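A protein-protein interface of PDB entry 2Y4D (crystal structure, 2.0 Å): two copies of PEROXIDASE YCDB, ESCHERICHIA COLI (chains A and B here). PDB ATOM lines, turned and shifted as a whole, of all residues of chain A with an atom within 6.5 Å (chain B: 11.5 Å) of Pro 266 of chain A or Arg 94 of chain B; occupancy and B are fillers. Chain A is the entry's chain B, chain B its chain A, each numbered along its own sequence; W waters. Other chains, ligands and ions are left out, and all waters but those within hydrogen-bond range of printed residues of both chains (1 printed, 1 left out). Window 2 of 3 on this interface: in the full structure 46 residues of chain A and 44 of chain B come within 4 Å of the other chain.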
ATOM      1  N   TRP A 262      23.628 -28.553  31.862  1.00  0.00           N
ATOM      2  CA  TRP A 262      22.671 -27.559  31.388  1.00  0.00           C
ATOM      3  C   TRP A 262      22.764 -27.352  29.886  1.00  0.00           C
ATOM      4  O   TRP A 262      21.738 -27.339  29.197  1.00  0.00           O
ATOM      5  CB  TRP A 262      22.891 -26.210  32.094  1.00  0.00           C
ATOM      6  CG  TRP A 262      21.898 -25.115  31.736  1.00  0.00           C
ATOM      7  CD1 TRP A 262      22.142 -23.993  30.992  1.00  0.00           C
ATOM      8  CD2 TRP A 262      20.527 -25.025  32.158  1.00  0.00           C
ATOM      9  NE1 TRP A 262      21.005 -23.219  30.904  1.00  0.00           N
ATOM     10  CE2 TRP A 262      20.000 -23.838  31.617  1.00  0.00           C
ATOM     11  CE3 TRP A 262      19.693 -25.844  32.948  1.00  0.00           C
ATOM     12  CZ2 TRP A 262      18.673 -23.425  31.850  1.00  0.00           C
ATOM     13  CZ3 TRP A 262      18.353 -25.421  33.198  1.00  0.00           C
ATOM     14  CH2 TRP A 262      17.868 -24.223  32.637  1.00  0.00           C
ATOM     15  N   ASP A 263      23.985 -27.176  29.376  1.00  0.00           N
ATOM     16  CA  ASP A 263      24.185 -26.902  27.942  1.00  0.00           C
ATOM     17  C   ASP A 263      23.857 -28.107  27.064  1.00  0.00           C
ATOM     18  O   ASP A 263      23.754 -27.957  25.850  1.00  0.00           O
ATOM     19  CB  ASP A 263      25.620 -26.429  27.616  1.00  0.00           C
ATOM     20  CG  ASP A 263      25.930 -25.002  28.163  1.00  0.00           C
ATOM     21  OD1 ASP A 263      24.989 -24.264  28.542  1.00  0.00           O
ATOM     22  OD2 ASP A 263      27.123 -24.616  28.173  1.00  0.00           O
ATOM     23  N   ARG A 264      23.727 -29.289  27.674  1.00  0.00           N
ATOM     24  CA  ARG A 264      23.286 -30.501  26.952  1.00  0.00           C
ATOM     25  C   ARG A 264      21.790 -30.732  27.085  1.00  0.00           C
ATOM     26  O   ARG A 264      21.295 -31.789  26.657  1.00  0.00           O
ATOM     27  CB  ARG A 264      24.032 -31.744  27.455  1.00  0.00           C
ATOM     28  CG  ARG A 264      25.313 -32.052  26.698  1.00  0.00           C
ATOM     29  CD  ARG A 264      25.881 -33.430  27.075  1.00  0.00           C
ATOM     30  NE  ARG A 264      26.433 -33.438  28.427  1.00  0.00           N
ATOM     31  CZ  ARG A 264      25.796 -33.893  29.501  1.00  0.00           C
ATOM     32  NH1 ARG A 264      24.569 -34.380  29.379  1.00  0.00           N
ATOM     33  NH2 ARG A 264      26.388 -33.858  30.699  1.00  0.00           N
ATOM     34  N   THR A 265      21.072 -29.768  27.670  1.00  0.00           N
ATOM     35  CA  THR A 265      19.659 -29.926  27.996  1.00  0.00           C
ATOM     36  C   THR A 265      18.798 -29.189  26.976  1.00  0.00           C
ATOM     37  O   THR A 265      19.128 -28.057  26.611  1.00  0.00           O
ATOM     38  CB  THR A 265      19.372 -29.432  29.423  1.00  0.00           C
ATOM     39  OG1 THR A 265      20.027 -30.294  30.360  1.00  0.00           O
ATOM     40  CG2 THR A 265      17.864 -29.369  29.756  1.00  0.00           C
ATOM     41  N   PRO A 266      17.718 -29.849  26.480  1.00  0.00           N
ATOM     42  CA  PRO A 266      16.835 -29.226  25.496  1.00  0.00           C
ATOM     43  C   PRO A 266      16.411 -27.819  25.895  1.00  0.00           C
ATOM     44  O   PRO A 266      16.157 -27.552  27.068  1.00  0.00           O
ATOM     45  CB  PRO A 266      15.620 -30.186  25.453  1.00  0.00           C
ATOM     46  CG  PRO A 266      16.225 -31.534  25.706  1.00  0.00           C
ATOM     47  CD  PRO A 266      17.432 -31.299  26.628  1.00  0.00           C
ATOM     48  N   LEU A 267      16.343 -26.908  24.929  1.00  0.00           N
ATOM     49  CA  LEU A 267      15.873 -25.550  25.233  1.00  0.00           C
ATOM     50  C   LEU A 267      14.446 -25.570  25.815  1.00  0.00           C
ATOM     51  O   LEU A 267      14.120 -24.823  26.760  1.00  0.00           O
ATOM     52  CB  LEU A 267      15.965 -24.684  23.963  1.00  0.00           C
ATOM     53  CG  LEU A 267      15.260 -23.315  23.986  1.00  0.00           C
ATOM     54  CD1 LEU A 267      15.868 -22.289  25.018  1.00  0.00           C
ATOM     55  CD2 LEU A 267      15.266 -22.730  22.562  1.00  0.00           C
ATOM     56  N   LYS A 268      13.588 -26.459  25.276  1.00  0.00           N
ATOM     57  CA  LYS A 268      12.209 -26.580  25.779  1.00  0.00           C
ATOM     58  C   LYS A 268      12.225 -26.856  27.292  1.00  0.00           C
ATOM     59  O   LYS A 268      11.539 -26.190  28.075  1.00  0.00           O
ATOM     60  CB  LYS A 268      11.513 -27.729  25.044  1.00  0.00           C
ATOM     61  CG  LYS A 268      10.026 -27.549  24.803  1.00  0.00           C
ATOM     62  CD  LYS A 268       9.445 -28.820  24.146  1.00  0.00           C
ATOM     63  CE  LYS A 268       8.074 -28.568  23.520  1.00  0.00           C
ATOM     64  NZ  LYS A 268       8.164 -28.344  22.046  1.00  0.00           N
ATOM     65  N   GLU A 269      13.063 -27.812  27.698  1.00  0.00           N
ATOM     66  CA  GLU A 269      13.211 -28.150  29.110  1.00  0.00           C
ATOM     67  C   GLU A 269      13.802 -26.976  29.915  1.00  0.00           C
ATOM     68  O   GLU A 269      13.386 -26.718  31.042  1.00  0.00           O
ATOM     69  CB  GLU A 269      14.082 -29.392  29.275  1.00  0.00           C
ATOM     70  CG  GLU A 269      14.098 -29.905  30.756  1.00  0.00           C
ATOM     71  CD  GLU A 269      14.928 -31.160  30.968  1.00  0.00           C
ATOM     72  OE1 GLU A 269      15.245 -31.860  29.964  1.00  0.00           O
ATOM     73  OE2 GLU A 269      15.277 -31.452  32.145  1.00  0.00           O
ATOM     74  N   GLN A 270      14.803 -26.285  29.353  1.00  0.00           N
ATOM     75  CA  GLN A 270      15.366 -25.107  30.054  1.00  0.00           C
ATOM     76  C   GLN A 270      14.262 -24.087  30.337  1.00  0.00           C
ATOM     77  O   GLN A 270      14.158 -23.519  31.452  1.00  0.00           O
ATOM     78  CB  GLN A 270      16.491 -24.446  29.219  1.00  0.00           C
ATOM     79  CG  GLN A 270      17.827 -25.253  29.182  1.00  0.00           C
ATOM     80  CD  GLN A 270      18.921 -24.436  28.475  1.00  0.00           C
ATOM     81  OE1 GLN A 270      18.708 -23.247  28.174  1.00  0.00           O
ATOM     82  NE2 GLN A 270      20.050 -25.068  28.157  1.00  0.00           N
ATOM     83  N   GLN A 271      13.432 -23.842  29.323  1.00  0.00           N
ATOM     84  CA  GLN A 271      12.349 -22.874  29.502  1.00  0.00           C
ATOM     85  C   GLN A 271      11.259 -23.372  30.462  1.00  0.00           C
ATOM     86  O   GLN A 271      10.738 -22.604  31.279  1.00  0.00           O
ATOM     87  CB  GLN A 271      11.795 -22.406  28.143  1.00  0.00           C
ATOM     88  CG  GLN A 271      12.848 -21.648  27.335  1.00  0.00           C
ATOM     89  CD  GLN A 271      12.334 -21.189  25.972  1.00  0.00           C
ATOM     90  OE1 GLN A 271      12.859 -20.228  25.398  1.00  0.00           O
ATOM     91  NE2 GLN A 271      11.289 -21.866  25.455  1.00  0.00           N
ATOM     92  N   TYR A 374      19.925 -28.865  38.521  1.00  0.00           N
ATOM     93  CA  TYR A 374      21.017 -28.168  37.856  1.00  0.00           C
ATOM     94  C   TYR A 374      21.785 -27.186  38.709  1.00  0.00           C
ATOM     95  O   TYR A 374      22.762 -26.597  38.221  1.00  0.00           O
ATOM     96  CB  TYR A 374      20.489 -27.430  36.629  1.00  0.00           C
ATOM     97  CG  TYR A 374      19.972 -28.365  35.584  1.00  0.00           C
ATOM     98  CD1 TYR A 374      20.818 -28.877  34.636  1.00  0.00           C
ATOM     99  CD2 TYR A 374      18.605 -28.735  35.550  1.00  0.00           C
ATOM    100  CE1 TYR A 374      20.337 -29.748  33.651  1.00  0.00           C
ATOM    101  CE2 TYR A 374      18.116 -29.607  34.571  1.00  0.00           C
ATOM    102  CZ  TYR A 374      18.999 -30.102  33.625  1.00  0.00           C
ATOM    103  OH  TYR A 374      18.577 -30.957  32.634  1.00  0.00           O
ATOM    104  N   GLU B  89      20.925 -20.122  15.925  1.00  0.00           N
ATOM    105  CA  GLU B  89      19.503 -20.206  16.248  1.00  0.00           C
ATOM    106  C   GLU B  89      19.142 -21.616  16.664  1.00  0.00           C
ATOM    107  O   GLU B  89      19.766 -22.567  16.235  1.00  0.00           O
ATOM    108  CB  GLU B  89      18.684 -19.883  14.996  1.00  0.00           C
ATOM    109  CG  GLU B  89      17.294 -19.395  15.295  1.00  0.00           C
ATOM    110  CD  GLU B  89      17.306 -17.951  15.744  1.00  0.00           C
ATOM    111  OE1 GLU B  89      17.826 -17.118  14.959  1.00  0.00           O
ATOM    112  OE2 GLU B  89      16.820 -17.660  16.873  1.00  0.00           O
ATOM    113  N   THR B  90      18.106 -21.745  17.484  1.00  0.00           N
ATOM    114  CA  THR B  90      17.607 -23.059  17.881  1.00  0.00           C
ATOM    115  C   THR B  90      16.165 -23.249  17.357  1.00  0.00           C
ATOM    116  O   THR B  90      15.209 -23.103  18.115  1.00  0.00           O
ATOM    117  CB  THR B  90      17.740 -23.243  19.423  1.00  0.00           C
ATOM    118  OG1 THR B  90      19.103 -22.980  19.789  1.00  0.00           O
ATOM    119  CG2 THR B  90      17.341 -24.679  19.890  1.00  0.00           C
ATOM    120  N   PRO B  91      16.013 -23.544  16.048  1.00  0.00           N
ATOM    121  CA  PRO B  91      14.643 -23.645  15.487  1.00  0.00           C
ATOM    122  C   PRO B  91      13.852 -24.866  16.019  1.00  0.00           C
ATOM    123  O   PRO B  91      12.637 -24.792  16.198  1.00  0.00           O
ATOM    124  CB  PRO B  91      14.878 -23.722  13.974  1.00  0.00           C
ATOM    125  CG  PRO B  91      16.275 -24.214  13.801  1.00  0.00           C
ATOM    126  CD  PRO B  91      17.057 -23.788  15.035  1.00  0.00           C
ATOM    127  N   ASN B  92      14.551 -25.953  16.304  1.00  0.00           N
ATOM    128  CA  ASN B  92      13.980 -27.114  16.989  1.00  0.00           C
ATOM    129  C   ASN B  92      14.275 -27.089  18.506  1.00  0.00           C
ATOM    130  O   ASN B  92      15.359 -27.506  18.925  1.00  0.00           O
ATOM    131  CB  ASN B  92      14.569 -28.402  16.382  1.00  0.00           C
ATOM    132  CG  ASN B  92      14.034 -29.681  17.049  1.00  0.00           C
ATOM    133  OD1 ASN B  92      13.136 -29.637  17.888  1.00  0.00           O
ATOM    134  ND2 ASN B  92      14.599 -30.825  16.671  1.00  0.00           N
ATOM    135  N   PRO B  93      13.299 -26.675  19.334  1.00  0.00           N
ATOM    136  CA  PRO B  93      13.578 -26.522  20.780  1.00  0.00           C
ATOM    137  C   PRO B  93      13.650 -27.826  21.576  1.00  0.00           C
ATOM    138  O   PRO B  93      13.830 -27.787  22.797  1.00  0.00           O
ATOM    139  CB  PRO B  93      12.411 -25.661  21.287  1.00  0.00           C
ATOM    140  CG  PRO B  93      11.288 -25.855  20.249  1.00  0.00           C
ATOM    141  CD  PRO B  93      11.865 -26.531  19.020  1.00  0.00           C
ATOM    142  N   ARG B  94      13.519 -28.970  20.903  1.00  0.00           N
ATOM    143  CA  ARG B  94      13.729 -30.257  21.552  1.00  0.00           C
ATOM    144  C   ARG B  94      15.217 -30.588  21.642  1.00  0.00           C
ATOM    145  O   ARG B  94      15.597 -31.533  22.329  1.00  0.00           O
ATOM    146  CB  ARG B  94      12.963 -31.385  20.830  1.00  0.00           C
ATOM    147  CG  ARG B  94      11.450 -31.266  20.966  1.00  0.00           C
ATOM    148  CD  ARG B  94      10.725 -32.426  20.268  1.00  0.00           C
ATOM    149  NE  ARG B  94      11.010 -32.468  18.828  1.00  0.00           N
ATOM    150  CZ  ARG B  94      10.465 -31.648  17.929  1.00  0.00           C
ATOM    151  NH1 ARG B  94       9.607 -30.708  18.300  1.00  0.00           N
ATOM    152  NH2 ARG B  94      10.775 -31.774  16.644  1.00  0.00           N
ATOM    153  N   LEU B  95      16.042 -29.806  20.935  1.00  0.00           N
ATOM    154  CA  LEU B  95      17.504 -29.927  20.957  1.00  0.00           C
ATOM    155  C   LEU B  95      18.072 -28.964  22.020  1.00  0.00           C
ATOM    156  O   LEU B  95      17.462 -27.920  22.298  1.00  0.00           O
ATOM    157  CB  LEU B  95      18.103 -29.599  19.564  1.00  0.00           C
ATOM    158  CG  LEU B  95      17.964 -30.621  18.406  1.00  0.00           C
ATOM    159  CD1 LEU B  95      18.557 -30.096  17.102  1.00  0.00           C
ATOM    160  CD2 LEU B  95      18.587 -31.976  18.784  1.00  0.00           C
ATOM    161  N   PRO B  96      19.226 -29.315  22.630  1.00  0.00           N
ATOM    162  CA  PRO B  96      19.937 -28.279  23.405  1.00  0.00           C
ATOM    163  C   PRO B  96      20.141 -27.006  22.545  1.00  0.00           C
ATOM    164  O   PRO B  96      20.382 -27.128  21.332  1.00  0.00           O
ATOM    165  CB  PRO B  96      21.296 -28.934  23.706  1.00  0.00           C
ATOM    166  CG  PRO B  96      21.040 -30.429  23.605  1.00  0.00           C
ATOM    167  CD  PRO B  96      19.973 -30.584  22.569  1.00  0.00           C
ATOM    168  N   PRO B  97      20.043 -25.805  23.165  1.00  0.00           N
ATOM    169  CA  PRO B  97      20.298 -24.571  22.401  1.00  0.00           C
ATOM    170  C   PRO B  97      21.667 -24.580  21.753  1.00  0.00           C
ATOM    171  O   PRO B  97      22.642 -25.037  22.376  1.00  0.00           O
ATOM    172  CB  PRO B  97      20.243 -23.449  23.464  1.00  0.00           C
ATOM    173  CG  PRO B  97      19.787 -24.082  24.749  1.00  0.00           C
ATOM    174  CD  PRO B  97      19.964 -25.563  24.624  1.00  0.00           C
ATOM    175  N   LEU B  98      21.747 -24.109  20.509  1.00  0.00           N
ATOM    176  CA  LEU B  98      23.019 -24.105  19.789  1.00  0.00           C
ATOM    177  C   LEU B  98      24.040 -23.144  20.402  1.00  0.00           C
ATOM    178  O   LEU B  98      25.218 -23.273  20.154  1.00  0.00           O
ATOM    179  CB  LEU B  98      22.828 -23.798  18.296  1.00  0.00           C
ATOM    180  CG  LEU B  98      22.016 -24.810  17.453  1.00  0.00           C
ATOM    181  CD1 LEU B  98      22.282 -24.579  15.967  1.00  0.00           C
ATOM    182  CD2 LEU B  98      22.389 -26.210  17.810  1.00  0.00           C
ATOM    183  N   ASP B  99      23.564 -22.214  21.213  1.00  0.00           N
ATOM    184  CA  ASP B  99      24.441 -21.273  21.929  1.00  0.00           C
ATOM    185  C   ASP B  99      23.949 -21.201  23.357  1.00  0.00           C
ATOM    186  O   ASP B  99      22.736 -21.308  23.601  1.00  0.00           O
ATOM    187  CB  ASP B  99      24.379 -19.883  21.268  1.00  0.00           C
ATOM    188  CG  ASP B  99      25.413 -18.892  21.845  1.00  0.00           C
ATOM    189  OD1 ASP B  99      26.608 -18.990  21.485  1.00  0.00           O
ATOM    190  OD2 ASP B  99      25.022 -18.012  22.638  1.00  0.00           O
ATOM    191  N   SER B 100      24.867 -20.975  24.309  1.00  0.00           N
ATOM    192  CA  SER B 100      24.519 -20.924  25.742  1.00  0.00           C
ATOM    193  C   SER B 100      23.609 -19.747  26.062  1.00  0.00           C
ATOM    194  O   SER B 100      22.939 -19.722  27.115  1.00  0.00           O
ATOM    195  CB  SER B 100      25.787 -20.793  26.583  1.00  0.00           C
ATOM    196  OG  SER B 100      26.530 -19.626  26.162  1.00  0.00           O
ATOM    197  N   LYS B 178      30.834 -27.575  24.589  1.00  0.00           N
ATOM    198  CA  LYS B 178      29.590 -28.128  23.987  1.00  0.00           C
ATOM    199  C   LYS B 178      29.857 -28.931  22.718  1.00  0.00           C
ATOM    200  O   LYS B 178      29.229 -29.988  22.469  1.00  0.00           O
ATOM    201  CB  LYS B 178      28.588 -27.016  23.672  1.00  0.00           C
ATOM    202  CG  LYS B 178      27.181 -27.505  23.285  1.00  0.00           C
ATOM    203  CD  LYS B 178      26.447 -26.511  22.398  1.00  0.00           C
ATOM    204  CE  LYS B 178      25.002 -27.004  22.143  1.00  0.00           C
ATOM    205  NZ  LYS B 178      24.962 -28.295  21.401  1.00  0.00           N
HETATM  206  O   HOH W   1      23.795 -25.138  24.776  1.00  0.00           O
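No position is printed for both chains. Of the 13 pairs that touch across the chains among the printed residues, none has its exchanged pair printed and touching as well.
The backbone carbonyl oxygen (O) of Pro 93 of chain B is in hydrogen-bond range of the backbone NH (N) of Leu 267 of chain A (3.4 Å). N of Lys 268 of chain A lies within hydrogen-bond range of O of Pro 93 of chain B. The backbone carbonyl oxygen of Leu 95 of chain B is in hydrogen-bond range of the backbone NH of Leu 267 of chain A.
Water W1 lies within hydrogen-bond range of the backbone carbonyl oxygen of Pro 97 of chain B (2.7 Å) and the backbone carbonyl oxygen of Asp 263 of chain A (3.0 Å).
Of the 13 printed residues of chain B, 6 touch a printed residue of chain A. Of the 11 printed residues of chain A, 7 touch a printed residue of chain B. Hydrophobic or aromatic side chains of chain A within 4 Å of the printed part of chain B: Pro 266 and Leu 267. Among the printed residues, 13 pairs touch across the chains. Among the printed residues, no Asp or Glu carboxylate lies within 4 Å of a Lys or Arg side-chain nitrogen of the other chain.
Printed residues of chain B within 4 Å of Pro 266 of chain A: Arg 94, Leu 95 and Pro 96. Of the printed residues of chain B, Leu 267 of chain A touches Thr 90, Pro 93, Leu 95 and Pro 97. Printed residues of chain B within 4 Å of Lys 268 of chain A: Pro 93. Glu 269 of chain A touches none of the printed residues of chain B. Tyr 374 of chain A touches none of the printed residues of chain B. Of the printed residues of chain A, Thr 90 of chain B touches Leu 267 (3.9 Å). Of the printed residues of chain A, Pro 93 of chain B touches Leu 267 and Lys 268. Arg 94 of chain B touches one residue of chain A. Lys 178 of chain B touches none of the printed residues of chain A. The nearest printed residue of chain B that does not touch Pro 266 of chain A is Pro 93 of chain B (4.002 Å). The nearest printed residue of chain A that does not touch Arg 94 of chain B is Lys 268 of chain A (4.5 Å).
Pro 96 of chain B touches Asp 263 of chain A. O of Arg 264 of chain A touches CG of Pro 96 of chain B (3.4 Å). Thr 265 of chain A touches Pro 96 of chain B (O to CA, 3.3 Å). O of Thr 265 of chain A touches CD of Pro 97 of chain B (3.3 Å). CB of Pro 266 of chain A touches O of Arg 94 of chain B, at 3.4 Å. O of Leu 95 of chain B touches CA of Pro 266 of chain A, at 3.5 Å. Pro 96 of chain B touches Pro 266 of chain A. CD2 of Leu 267 of chain A touches CG2 of Thr 90 of chain B, 3.9 Å away. Leu 267 of chain A touches Pro 97 of chain B (N to CD, 3.9 Å). Pro 97 of chain B touches Gln 270 of chain A (CG to NE2, 3.6 Å).
N of Leu 98 of chain B lies within hydrogen-bond range of OG1 of Thr 90 of chain B (3.0 Å). OD1 of Asn 92 of chain B sits at hydrogen-bond distance from N of Arg 94 of chain B. O of Trp 262 of chain A lies within hydrogen-bond range of NE2 of Gln 270 of chain A (3.0 Å). The side-chain amide nitrogen of Gln 270 of chain A is in hydrogen-bond range of the backbone carbonyl oxygen of Thr 265 of chain A, 3.5 Å away. The side-chain hydroxyl of Tyr 374 of chain A is in hydrogen-bond range of the side-chain hydroxyl of Thr 265 of chain A, at 2.8 Å.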
